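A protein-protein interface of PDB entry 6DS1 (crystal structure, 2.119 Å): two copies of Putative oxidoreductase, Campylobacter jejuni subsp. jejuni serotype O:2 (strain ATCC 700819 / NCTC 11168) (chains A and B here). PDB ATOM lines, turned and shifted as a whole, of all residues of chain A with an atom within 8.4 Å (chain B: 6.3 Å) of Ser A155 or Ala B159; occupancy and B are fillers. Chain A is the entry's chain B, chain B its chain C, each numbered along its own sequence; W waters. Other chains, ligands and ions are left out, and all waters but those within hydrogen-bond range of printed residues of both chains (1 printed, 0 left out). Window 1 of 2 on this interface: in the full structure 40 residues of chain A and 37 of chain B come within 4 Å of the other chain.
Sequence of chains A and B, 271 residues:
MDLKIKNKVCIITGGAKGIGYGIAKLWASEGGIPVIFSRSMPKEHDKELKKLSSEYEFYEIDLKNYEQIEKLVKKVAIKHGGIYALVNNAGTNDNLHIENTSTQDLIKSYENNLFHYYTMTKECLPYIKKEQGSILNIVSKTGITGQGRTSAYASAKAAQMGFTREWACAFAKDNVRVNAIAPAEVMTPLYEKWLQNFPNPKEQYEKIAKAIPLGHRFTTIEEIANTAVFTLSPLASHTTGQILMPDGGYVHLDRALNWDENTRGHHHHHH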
ATOM      1  N   LEU A  96      -1.227  25.220 -14.993  1.00  0.00           N
ATOM      2  CA  LEU A  96      -1.809  26.553 -15.130  1.00  0.00           C
ATOM      3  C   LEU A  96      -0.647  27.528 -15.281  1.00  0.00           C
ATOM      4  O   LEU A  96       0.066  27.820 -14.317  1.00  0.00           O
ATOM      5  CB  LEU A  96      -2.719  26.889 -13.943  1.00  0.00           C
ATOM      6  CG  LEU A  96      -3.927  25.950 -13.769  1.00  0.00           C
ATOM      7  CD1 LEU A  96      -4.780  26.346 -12.561  1.00  0.00           C
ATOM      8  CD2 LEU A  96      -4.798  25.861 -15.054  1.00  0.00           C
ATOM      9  N   LEU A 106      -6.003  30.847 -10.362  1.00  0.00           N
ATOM     10  CA  LEU A 106      -4.925  30.447  -9.461  1.00  0.00           C
ATOM     11  C   LEU A 106      -5.481  30.099  -8.086  1.00  0.00           C
ATOM     12  O   LEU A 106      -5.115  29.079  -7.487  1.00  0.00           O
ATOM     13  CB  LEU A 106      -3.874  31.556  -9.342  1.00  0.00           C
ATOM     14  CG  LEU A 106      -2.819  31.338  -8.252  1.00  0.00           C
ATOM     15  CD1 LEU A 106      -1.597  30.576  -8.798  1.00  0.00           C
ATOM     16  CD2 LEU A 106      -2.411  32.657  -7.605  1.00  0.00           C
ATOM     17  N   SER A 109      -7.119  26.812  -8.019  1.00  0.00           N
ATOM     18  CA  SER A 109      -6.101  25.765  -7.953  1.00  0.00           C
ATOM     19  C   SER A 109      -5.654  25.540  -6.517  1.00  0.00           C
ATOM     20  O   SER A 109      -5.491  24.394  -6.082  1.00  0.00           O
ATOM     21  CB  SER A 109      -4.905  26.130  -8.843  1.00  0.00           C
ATOM     22  OG  SER A 109      -3.973  25.057  -8.950  1.00  0.00           O
ATOM     23  N   TYR A 110      -5.461  26.625  -5.763  1.00  0.00           N
ATOM     24  CA  TYR A 110      -5.034  26.497  -4.372  1.00  0.00           C
ATOM     25  C   TYR A 110      -6.111  25.816  -3.528  1.00  0.00           C
ATOM     26  O   TYR A 110      -5.793  25.060  -2.599  1.00  0.00           O
ATOM     27  CB  TYR A 110      -4.684  27.876  -3.791  1.00  0.00           C
ATOM     28  CG  TYR A 110      -3.394  28.513  -4.305  1.00  0.00           C
ATOM     29  CD1 TYR A 110      -2.464  27.792  -5.063  1.00  0.00           C
ATOM     30  CD2 TYR A 110      -3.098  29.838  -4.013  1.00  0.00           C
ATOM     31  CE1 TYR A 110      -1.292  28.388  -5.519  1.00  0.00           C
ATOM     32  CE2 TYR A 110      -1.932  30.432  -4.464  1.00  0.00           C
ATOM     33  CZ  TYR A 110      -1.028  29.706  -5.209  1.00  0.00           C
ATOM     34  OH  TYR A 110       0.131  30.322  -5.644  1.00  0.00           O
ATOM     35  N   ASN A 113      -5.477  22.210  -4.363  1.00  0.00           N
ATOM     36  CA  ASN A 113      -4.157  21.655  -4.129  1.00  0.00           C
ATOM     37  C   ASN A 113      -3.528  22.066  -2.809  1.00  0.00           C
ATOM     38  O   ASN A 113      -2.630  21.365  -2.344  1.00  0.00           O
ATOM     39  CB  ASN A 113      -3.192  22.073  -5.250  1.00  0.00           C
ATOM     40  CG  ASN A 113      -3.387  21.276  -6.526  1.00  0.00           C
ATOM     41  OD1 ASN A 113      -4.021  20.217  -6.532  1.00  0.00           O
ATOM     42  ND2 ASN A 113      -2.838  21.786  -7.621  1.00  0.00           N
ATOM     43  N   LEU A 114      -3.944  23.186  -2.209  1.00  0.00           N
ATOM     44  CA  LEU A 114      -3.126  23.810  -1.174  1.00  0.00           C
ATOM     45  C   LEU A 114      -3.842  23.982   0.152  1.00  0.00           C
ATOM     46  O   LEU A 114      -3.304  23.564   1.179  1.00  0.00           O
ATOM     47  CB  LEU A 114      -2.604  25.178  -1.643  1.00  0.00           C
ATOM     48  CG  LEU A 114      -1.862  25.982  -0.571  1.00  0.00           C
ATOM     49  CD1 LEU A 114      -0.699  25.160   0.012  1.00  0.00           C
ATOM     50  CD2 LEU A 114      -1.369  27.338  -1.135  1.00  0.00           C
ATOM     51  N   THR A 142       8.819  20.164  -8.611  1.00  0.00           N
ATOM     52  CA  THR A 142       8.542  21.410  -9.308  1.00  0.00           C
ATOM     53  C   THR A 142       8.555  22.594  -8.358  1.00  0.00           C
ATOM     54  O   THR A 142       8.882  23.711  -8.774  1.00  0.00           O
ATOM     55  CB  THR A 142       7.207  21.279 -10.033  1.00  0.00           C
ATOM     56  OG1 THR A 142       7.324  20.218 -10.989  1.00  0.00           O
ATOM     57  CG2 THR A 142       6.840  22.574 -10.763  1.00  0.00           C
ATOM     58  N   GLY A 143       8.228  22.362  -7.083  1.00  0.00           N
ATOM     59  CA  GLY A 143       8.361  23.377  -6.055  1.00  0.00           C
ATOM     60  C   GLY A 143       9.786  23.842  -5.841  1.00  0.00           C
ATOM     61  O   GLY A 143       9.994  24.956  -5.354  1.00  0.00           O
ATOM     62  N   ILE A 144      10.769  23.034  -6.235  1.00  0.00           N
ATOM     63  CA  ILE A 144      12.190  23.339  -6.043  1.00  0.00           C
ATOM     64  C   ILE A 144      12.843  23.803  -7.337  1.00  0.00           C
ATOM     65  O   ILE A 144      13.588  24.780  -7.352  1.00  0.00           O
ATOM     66  CB  ILE A 144      12.926  22.103  -5.479  1.00  0.00           C
ATOM     67  CG1 ILE A 144      12.351  21.687  -4.131  1.00  0.00           C
ATOM     68  CG2 ILE A 144      14.421  22.355  -5.367  1.00  0.00           C
ATOM     69  CD1 ILE A 144      12.380  20.176  -3.917  1.00  0.00           C
ATOM     70  N   GLY A 146      11.144  24.320 -10.390  1.00  0.00           N
ATOM     71  CA  GLY A 146      10.253  24.892 -11.373  1.00  0.00           C
ATOM     72  C   GLY A 146      10.014  23.919 -12.510  1.00  0.00           C
ATOM     73  O   GLY A 146      10.602  22.835 -12.569  1.00  0.00           O
ATOM     74  N   THR A 150       3.498  25.827 -15.246  1.00  0.00           N
ATOM     75  CA  THR A 150       2.593  25.344 -14.207  1.00  0.00           C
ATOM     76  C   THR A 150       2.804  26.192 -12.941  1.00  0.00           C
ATOM     77  O   THR A 150       3.261  25.752 -11.886  1.00  0.00           O
ATOM     78  CB  THR A 150       2.793  23.836 -14.003  1.00  0.00           C
ATOM     79  OG1 THR A 150       1.768  23.299 -13.154  1.00  0.00           O
ATOM     80  CG2 THR A 150       4.190  23.506 -13.453  1.00  0.00           C
ATOM     81  N   SER A 151       2.446  27.476 -13.045  1.00  0.00           N
ATOM     82  CA  SER A 151       2.677  28.427 -11.955  1.00  0.00           C
ATOM     83  C   SER A 151       1.900  28.052 -10.701  1.00  0.00           C
ATOM     84  O   SER A 151       2.423  28.154  -9.585  1.00  0.00           O
ATOM     85  CB  SER A 151       2.296  29.846 -12.397  1.00  0.00           C
ATOM     86  OG  SER A 151       3.418  30.556 -12.888  1.00  0.00           O
ATOM     87  N   ALA A 152       0.638  27.630 -10.862  1.00  0.00           N
ATOM     88  CA  ALA A 152      -0.206  27.349  -9.703  1.00  0.00           C
ATOM     89  C   ALA A 152       0.304  26.148  -8.923  1.00  0.00           C
ATOM     90  O   ALA A 152       0.319  26.163  -7.684  1.00  0.00           O
ATOM     91  CB  ALA A 152      -1.655  27.122 -10.146  1.00  0.00           C
ATOM     92  N   TYR A 153       0.723  25.096  -9.629  1.00  0.00           N
ATOM     93  CA  TYR A 153       1.137  23.862  -8.962  1.00  0.00           C
ATOM     94  C   TYR A 153       2.516  24.009  -8.323  1.00  0.00           C
ATOM     95  O   TYR A 153       2.758  23.483  -7.227  1.00  0.00           O
ATOM     96  CB  TYR A 153       1.105  22.720  -9.975  1.00  0.00           C
ATOM     97  CG  TYR A 153       1.600  21.379  -9.484  1.00  0.00           C
ATOM     98  CD1 TYR A 153       0.819  20.581  -8.645  1.00  0.00           C
ATOM     99  CD2 TYR A 153       2.844  20.893  -9.884  1.00  0.00           C
ATOM    100  CE1 TYR A 153       1.265  19.336  -8.226  1.00  0.00           C
ATOM    101  CE2 TYR A 153       3.298  19.650  -9.464  1.00  0.00           C
ATOM    102  CZ  TYR A 153       2.505  18.880  -8.639  1.00  0.00           C
ATOM    103  OH  TYR A 153       2.962  17.647  -8.228  1.00  0.00           O
ATOM    104  N   ALA A 154       3.414  24.770  -8.964  1.00  0.00           N
ATOM    105  CA  ALA A 154       4.765  24.952  -8.432  1.00  0.00           C
ATOM    106  C   ALA A 154       4.747  25.753  -7.139  1.00  0.00           C
ATOM    107  O   ALA A 154       5.432  25.400  -6.170  1.00  0.00           O
ATOM    108  CB  ALA A 154       5.656  25.645  -9.465  1.00  0.00           C
ATOM    109  N   SER A 155       3.986  26.849  -7.112  1.00  0.00           N
ATOM    110  CA  SER A 155       3.926  27.660  -5.900  1.00  0.00           C
ATOM    111  C   SER A 155       3.189  26.933  -4.782  1.00  0.00           C
ATOM    112  O   SER A 155       3.557  27.059  -3.606  1.00  0.00           O
ATOM    113  CB  SER A 155       3.278  29.018  -6.184  1.00  0.00           C
ATOM    114  OG  SER A 155       2.027  28.895  -6.829  1.00  0.00           O
ATOM    115  N   ALA A 156       2.151  26.159  -5.122  1.00  0.00           N
ATOM    116  CA  ALA A 156       1.458  25.388  -4.087  1.00  0.00           C
ATOM    117  C   ALA A 156       2.397  24.357  -3.468  1.00  0.00           C
ATOM    118  O   ALA A 156       2.459  24.221  -2.240  1.00  0.00           O
ATOM    119  CB  ALA A 156       0.206  24.710  -4.659  1.00  0.00           C
ATOM    120  N   LYS A 157       3.159  23.647  -4.305  1.00  0.00           N
ATOM    121  CA  LYS A 157       4.095  22.648  -3.795  1.00  0.00           C
ATOM    122  C   LYS A 157       5.221  23.296  -2.990  1.00  0.00           C
ATOM    123  O   LYS A 157       5.635  22.764  -1.955  1.00  0.00           O
ATOM    124  CB  LYS A 157       4.639  21.819  -4.955  1.00  0.00           C
ATOM    125  CG  LYS A 157       3.566  20.908  -5.553  1.00  0.00           C
ATOM    126  CD  LYS A 157       3.031  19.960  -4.475  1.00  0.00           C
ATOM    127  CE  LYS A 157       1.556  19.647  -4.638  1.00  0.00           C
ATOM    128  NZ  LYS A 157       1.159  18.459  -3.792  1.00  0.00           N
ATOM    129  N   ALA A 158       5.712  24.457  -3.432  1.00  0.00           N
ATOM    130  CA  ALA A 158       6.687  25.188  -2.633  1.00  0.00           C
ATOM    131  C   ALA A 158       6.070  25.675  -1.319  1.00  0.00           C
ATOM    132  O   ALA A 158       6.696  25.563  -0.256  1.00  0.00           O
ATOM    133  CB  ALA A 158       7.256  26.351  -3.447  1.00  0.00           C
ATOM    134  N   ALA A 159       4.827  26.180  -1.363  1.00  0.00           N
ATOM    135  CA  ALA A 159       4.137  26.569  -0.130  1.00  0.00           C
ATOM    136  C   ALA A 159       4.125  25.431   0.885  1.00  0.00           C
ATOM    137  O   ALA A 159       4.329  25.651   2.088  1.00  0.00           O
ATOM    138  CB  ALA A 159       2.698  27.006  -0.434  1.00  0.00           C
ATOM    139  N   GLN A 160       3.885  24.201   0.411  1.00  0.00           N
ATOM    140  CA  GLN A 160       3.839  23.046   1.298  1.00  0.00           C
ATOM    141  C   GLN A 160       5.211  22.719   1.882  1.00  0.00           C
ATOM    142  O   GLN A 160       5.294  22.146   2.977  1.00  0.00           O
ATOM    143  CB  GLN A 160       3.249  21.845   0.544  1.00  0.00           C
ATOM    144  CG  GLN A 160       1.821  22.103   0.036  1.00  0.00           C
ATOM    145  CD  GLN A 160       1.355  21.085  -1.003  1.00  0.00           C
ATOM    146  OE1 GLN A 160       2.100  20.187  -1.385  1.00  0.00           O
ATOM    147  NE2 GLN A 160       0.101  21.204  -1.431  1.00  0.00           N
ATOM    148  N   MET A 161       6.293  23.079   1.187  1.00  0.00           N
ATOM    149  CA  MET A 161       7.620  22.939   1.787  1.00  0.00           C
ATOM    150  C   MET A 161       7.809  23.930   2.921  1.00  0.00           C
ATOM    151  O   MET A 161       8.416  23.597   3.949  1.00  0.00           O
ATOM    152  CB  MET A 161       8.705  23.128   0.729  1.00  0.00           C
ATOM    153  CG  MET A 161       8.539  22.137  -0.395  1.00  0.00           C
ATOM    154  SD  MET A 161       9.905  22.097  -1.546  1.00  0.00           S
ATOM    155  CE  MET A 161       9.089  21.277  -2.928  1.00  0.00           C
ATOM    156  N   GLY A 162       7.309  25.157   2.746  1.00  0.00           N
ATOM    157  CA  GLY A 162       7.340  26.114   3.844  1.00  0.00           C
ATOM    158  C   GLY A 162       6.515  25.658   5.032  1.00  0.00           C
ATOM    159  O   GLY A 162       6.935  25.805   6.183  1.00  0.00           O
ATOM    160  N   PHE A 163       5.317  25.114   4.769  1.00  0.00           N
ATOM    161  CA  PHE A 163       4.517  24.489   5.823  1.00  0.00           C
ATOM    162  C   PHE A 163       5.312  23.399   6.541  1.00  0.00           C
ATOM    163  O   PHE A 163       5.259  23.288   7.770  1.00  0.00           O
ATOM    164  CB  PHE A 163       3.235  23.890   5.234  1.00  0.00           C
ATOM    165  CG  PHE A 163       2.094  24.873   5.065  1.00  0.00           C
ATOM    166  CD1 PHE A 163       1.897  25.914   5.956  1.00  0.00           C
ATOM    167  CD2 PHE A 163       1.189  24.723   4.023  1.00  0.00           C
ATOM    168  CE1 PHE A 163       0.816  26.792   5.803  1.00  0.00           C
ATOM    169  CE2 PHE A 163       0.109  25.596   3.859  1.00  0.00           C
ATOM    170  CZ  PHE A 163      -0.069  26.631   4.748  1.00  0.00           C
ATOM    171  N   LEU B 114       0.439  37.330  -0.926  1.00  0.00           N
ATOM    172  CA  LEU B 114       0.870  36.349  -1.908  1.00  0.00           C
ATOM    173  C   LEU B 114       0.299  36.597  -3.296  1.00  0.00           C
ATOM    174  O   LEU B 114       1.064  36.670  -4.267  1.00  0.00           O
ATOM    175  CB  LEU B 114       0.490  34.938  -1.442  1.00  0.00           C
ATOM    176  CG  LEU B 114       0.855  33.837  -2.441  1.00  0.00           C
ATOM    177  CD1 LEU B 114       2.337  33.901  -2.776  1.00  0.00           C
ATOM    178  CD2 LEU B 114       0.474  32.464  -1.923  1.00  0.00           C
ATOM    179  N   ALA B 154       5.033  32.034   6.503  1.00  0.00           N
ATOM    180  CA  ALA B 154       6.061  31.089   6.067  1.00  0.00           C
ATOM    181  C   ALA B 154       5.668  30.416   4.757  1.00  0.00           C
ATOM    182  O   ALA B 154       6.505  30.239   3.863  1.00  0.00           O
ATOM    183  CB  ALA B 154       6.323  30.034   7.149  1.00  0.00           C
ATOM    184  N   SER B 155       4.399  30.023   4.633  1.00  0.00           N
ATOM    185  CA  SER B 155       3.955  29.332   3.427  1.00  0.00           C
ATOM    186  C   SER B 155       3.916  30.282   2.236  1.00  0.00           C
ATOM    187  O   SER B 155       4.349  29.922   1.134  1.00  0.00           O
ATOM    188  CB  SER B 155       2.590  28.674   3.667  1.00  0.00           C
ATOM    189  OG  SER B 155       1.598  29.609   4.085  1.00  0.00           O
ATOM    190  N   ALA B 156       3.456  31.523   2.449  1.00  0.00           N
ATOM    191  CA  ALA B 156       3.445  32.512   1.368  1.00  0.00           C
ATOM    192  C   ALA B 156       4.854  32.783   0.836  1.00  0.00           C
ATOM    193  O   ALA B 156       5.067  32.840  -0.382  1.00  0.00           O
ATOM    194  CB  ALA B 156       2.793  33.813   1.852  1.00  0.00           C
ATOM    195  N   LYS B 157       5.834  32.941   1.732  1.00  0.00           N
ATOM    196  CA  LYS B 157       7.184  33.270   1.287  1.00  0.00           C
ATOM    197  C   LYS B 157       7.829  32.080   0.583  1.00  0.00           C
ATOM    198  O   LYS B 157       8.536  32.249  -0.418  1.00  0.00           O
ATOM    199  CB  LYS B 157       8.019  33.744   2.480  1.00  0.00           C
ATOM    200  CG  LYS B 157       7.428  34.979   3.178  1.00  0.00           C
ATOM    201  CD  LYS B 157       7.891  36.280   2.514  1.00  0.00           C
ATOM    202  CE  LYS B 157       6.721  37.195   2.129  1.00  0.00           C
ATOM    203  NZ  LYS B 157       7.175  38.398   1.355  1.00  0.00           N
ATOM    204  N   ALA B 158       7.568  30.869   1.078  1.00  0.00           N
ATOM    205  CA  ALA B 158       8.006  29.673   0.377  1.00  0.00           C
ATOM    206  C   ALA B 158       7.348  29.569  -0.995  1.00  0.00           C
ATOM    207  O   ALA B 158       8.005  29.205  -1.980  1.00  0.00           O
ATOM    208  CB  ALA B 158       7.695  28.440   1.219  1.00  0.00           C
ATOM    209  N   ALA B 159       6.055  29.890  -1.082  1.00  0.00           N
ATOM    210  CA  ALA B 159       5.387  29.910  -2.385  1.00  0.00           C
ATOM    211  C   ALA B 159       6.076  30.879  -3.340  1.00  0.00           C
ATOM    212  O   ALA B 159       6.236  30.581  -4.532  1.00  0.00           O
ATOM    213  CB  ALA B 159       3.910  30.276  -2.222  1.00  0.00           C
ATOM    214  N   GLN B 160       6.522  32.030  -2.826  1.00  0.00           N
ATOM    215  CA  GLN B 160       7.235  32.993  -3.663  1.00  0.00           C
ATOM    216  C   GLN B 160       8.577  32.446  -4.143  1.00  0.00           C
ATOM    217  O   GLN B 160       9.027  32.790  -5.247  1.00  0.00           O
ATOM    218  CB  GLN B 160       7.393  34.308  -2.900  1.00  0.00           C
ATOM    219  CG  GLN B 160       6.038  34.948  -2.565  1.00  0.00           C
ATOM    220  CD  GLN B 160       6.119  36.068  -1.530  1.00  0.00           C
ATOM    221  OE1 GLN B 160       7.186  36.366  -0.982  1.00  0.00           O
ATOM    222  NE2 GLN B 160       4.977  36.708  -1.272  1.00  0.00           N
ATOM    223  N   MET B 161       9.217  31.567  -3.360  1.00  0.00           N
ATOM    224  CA  MET B 161      10.398  30.870  -3.871  1.00  0.00           C
ATOM    225  C   MET B 161      10.033  29.928  -5.016  1.00  0.00           C
ATOM    226  O   MET B 161      10.760  29.851  -6.019  1.00  0.00           O
ATOM    227  CB  MET B 161      11.096  30.118  -2.736  1.00  0.00           C
ATOM    228  CG  MET B 161      11.725  31.068  -1.727  1.00  0.00           C
ATOM    229  SD  MET B 161      12.357  30.235  -0.278  1.00  0.00           S
ATOM    230  CE  MET B 161      12.146  31.552   0.927  1.00  0.00           C
ATOM    231  N   GLY B 162       8.902  29.218  -4.891  1.00  0.00           N
ATOM    232  CA  GLY B 162       8.409  28.419  -6.007  1.00  0.00           C
ATOM    233  C   GLY B 162       8.154  29.254  -7.251  1.00  0.00           C
ATOM    234  O   GLY B 162       8.572  28.891  -8.358  1.00  0.00           O
ATOM    235  N   PHE B 163       7.467  30.388  -7.081  1.00  0.00           N
ATOM    236  CA  PHE B 163       7.250  31.308  -8.195  1.00  0.00           C
ATOM    237  C   PHE B 163       8.580  31.720  -8.820  1.00  0.00           C
ATOM    238  O   PHE B 163       8.693  31.815 -10.045  1.00  0.00           O
ATOM    239  CB  PHE B 163       6.478  32.545  -7.721  1.00  0.00           C
ATOM    240  CG  PHE B 163       4.981  32.362  -7.661  1.00  0.00           C
ATOM    241  CD1 PHE B 163       4.314  31.589  -8.607  1.00  0.00           C
ATOM    242  CD2 PHE B 163       4.236  32.979  -6.664  1.00  0.00           C
ATOM    243  CE1 PHE B 163       2.932  31.437  -8.559  1.00  0.00           C
ATOM    244  CE2 PHE B 163       2.855  32.827  -6.608  1.00  0.00           C
ATOM    245  CZ  PHE B 163       2.208  32.054  -7.550  1.00  0.00           C
ATOM    246  N   THR B 164       9.606  31.925  -7.992  1.00  0.00           N
ATOM    247  CA  THR B 164      10.890  32.396  -8.498  1.00  0.00           C
ATOM    248  C   THR B 164      11.516  31.380  -9.440  1.00  0.00           C
ATOM    249  O   THR B 164      11.974  31.728 -10.535  1.00  0.00           O
ATOM    250  CB  THR B 164      11.841  32.684  -7.342  1.00  0.00           C
ATOM    251  OG1 THR B 164      11.295  33.719  -6.515  1.00  0.00           O
ATOM    252  CG2 THR B 164      13.184  33.123  -7.891  1.00  0.00           C
ATOM    253  N   GLU B 166       9.916  28.763 -10.858  1.00  0.00           N
ATOM    254  CA  GLU B 166       8.997  28.464 -11.946  1.00  0.00           C
ATOM    255  C   GLU B 166       9.069  29.536 -13.024  1.00  0.00           C
ATOM    256  O   GLU B 166       9.184  29.228 -14.215  1.00  0.00           O
ATOM    257  CB  GLU B 166       7.575  28.348 -11.403  1.00  0.00           C
ATOM    258  CG  GLU B 166       6.520  28.468 -12.484  1.00  0.00           C
ATOM    259  CD  GLU B 166       6.486  27.243 -13.371  1.00  0.00           C
ATOM    260  OE1 GLU B 166       7.142  26.239 -13.013  1.00  0.00           O
ATOM    261  OE2 GLU B 166       5.811  27.283 -14.422  1.00  0.00           O
HETATM  262  O   HOH W   1       3.981  29.305 -15.300  1.00  0.00           O
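Leu A114 touches none of the printed residues of chain B. Of the printed residues of chain B, Gly A146 touches Glu B166 (3.7 Å). Of chain B, only Ala B159 and Phe B163 come within 4 Å of Ser A155. Ala A156 touches none of the printed residues of chain B. Of the printed residues of chain B, Ala A158 touches Ala B158 (3.3 Å) and Gly B162 (3.5 Å). Printed residues of chain B within 4 Å of Gly A162: Ala B158 (3.5 Å). Ala B158 touches just these residues of chain A: Ala A158 (3.3 Å) and Gly A162 (3.5 Å). The nearest residue of chain B that does not touch Ser A155 is Gly B162 (4.5 Å). The nearest printed residue of chain A that does not touch Gly B162 is Ala A154 (4.2 Å).
OE2 of Glu B166 sits at hydrogen-bond distance from N of Thr A150.
Water W1 bridges the side-chain hydroxyl (OG) of Ser A151 (2.8 Å) and the side-chain carboxylate (OE2) of Glu B166 (2.9 Å).
The backbone NH (N) of Ser A151 is in hydrogen-bond range of the backbone carbonyl oxygen (O) of Leu A96 (2.7 Å). OG of Ser A155 sits at hydrogen-bond distance from OH of Tyr A110 (2.7 Å). The backbone carbonyl oxygen of Ser A151 sits at hydrogen-bond distance from the side-chain hydroxyl of Ser A155 (2.9 Å). O of Ala A152 lies within hydrogen-bond range of OG of Ser A155 (3.3 Å).
Hydrophobic or aromatic side chains of chain A that line the printed part of chain B: Tyr A110, Ala A154, Ala A158, Ala A159 and Phe A163. Along chain A the printed residues that touch a printed residue of chain B span positions 110 to 163. Of the 13 printed residues of chain B, 6 touch a printed residue of chain A. Among the printed residues, no Asp or Glu carboxylate lies within 4 Å of a Lys or Arg side-chain nitrogen of the other chain.
Gly A143 touches Gly B162 (O to CA, 3.9 Å). Phe B163 touches Ser A151. CB of Ala A154 touches CB of Glu B166 (3.8 Å). Ser A155 touches Ala B159 (O to CB, 3.5 Å). Phe B163 touches Ser A155 (CE1 to OG, 3.2 Å). CB of Ala A158 touches CA of Gly B162 (3.5 Å). Ala A159 touches Ser B155 (CA to O, 3.6 Å). Ala A159 touches Ala B159. Ala B158 touches Gly A162 (CB to CA, 3.5 Å). Phe A163 touches Ser B155 (CE1 to CB, 3.4 Å).
Ser A155 touches Phe B163, and with the chains exchanged Phe A163 touches Ser B155. Ala A158 touches its own counterpart, Ala B158. Ala A158 touches Gly B162, and with the chains exchanged Gly A162 touches Ala B158. Ala B159 touches its own counterpart, Ala A159. Of the 15 pairs that touch across the chains among the printed residues, 8 have their exchanged pair printed and touching as well.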
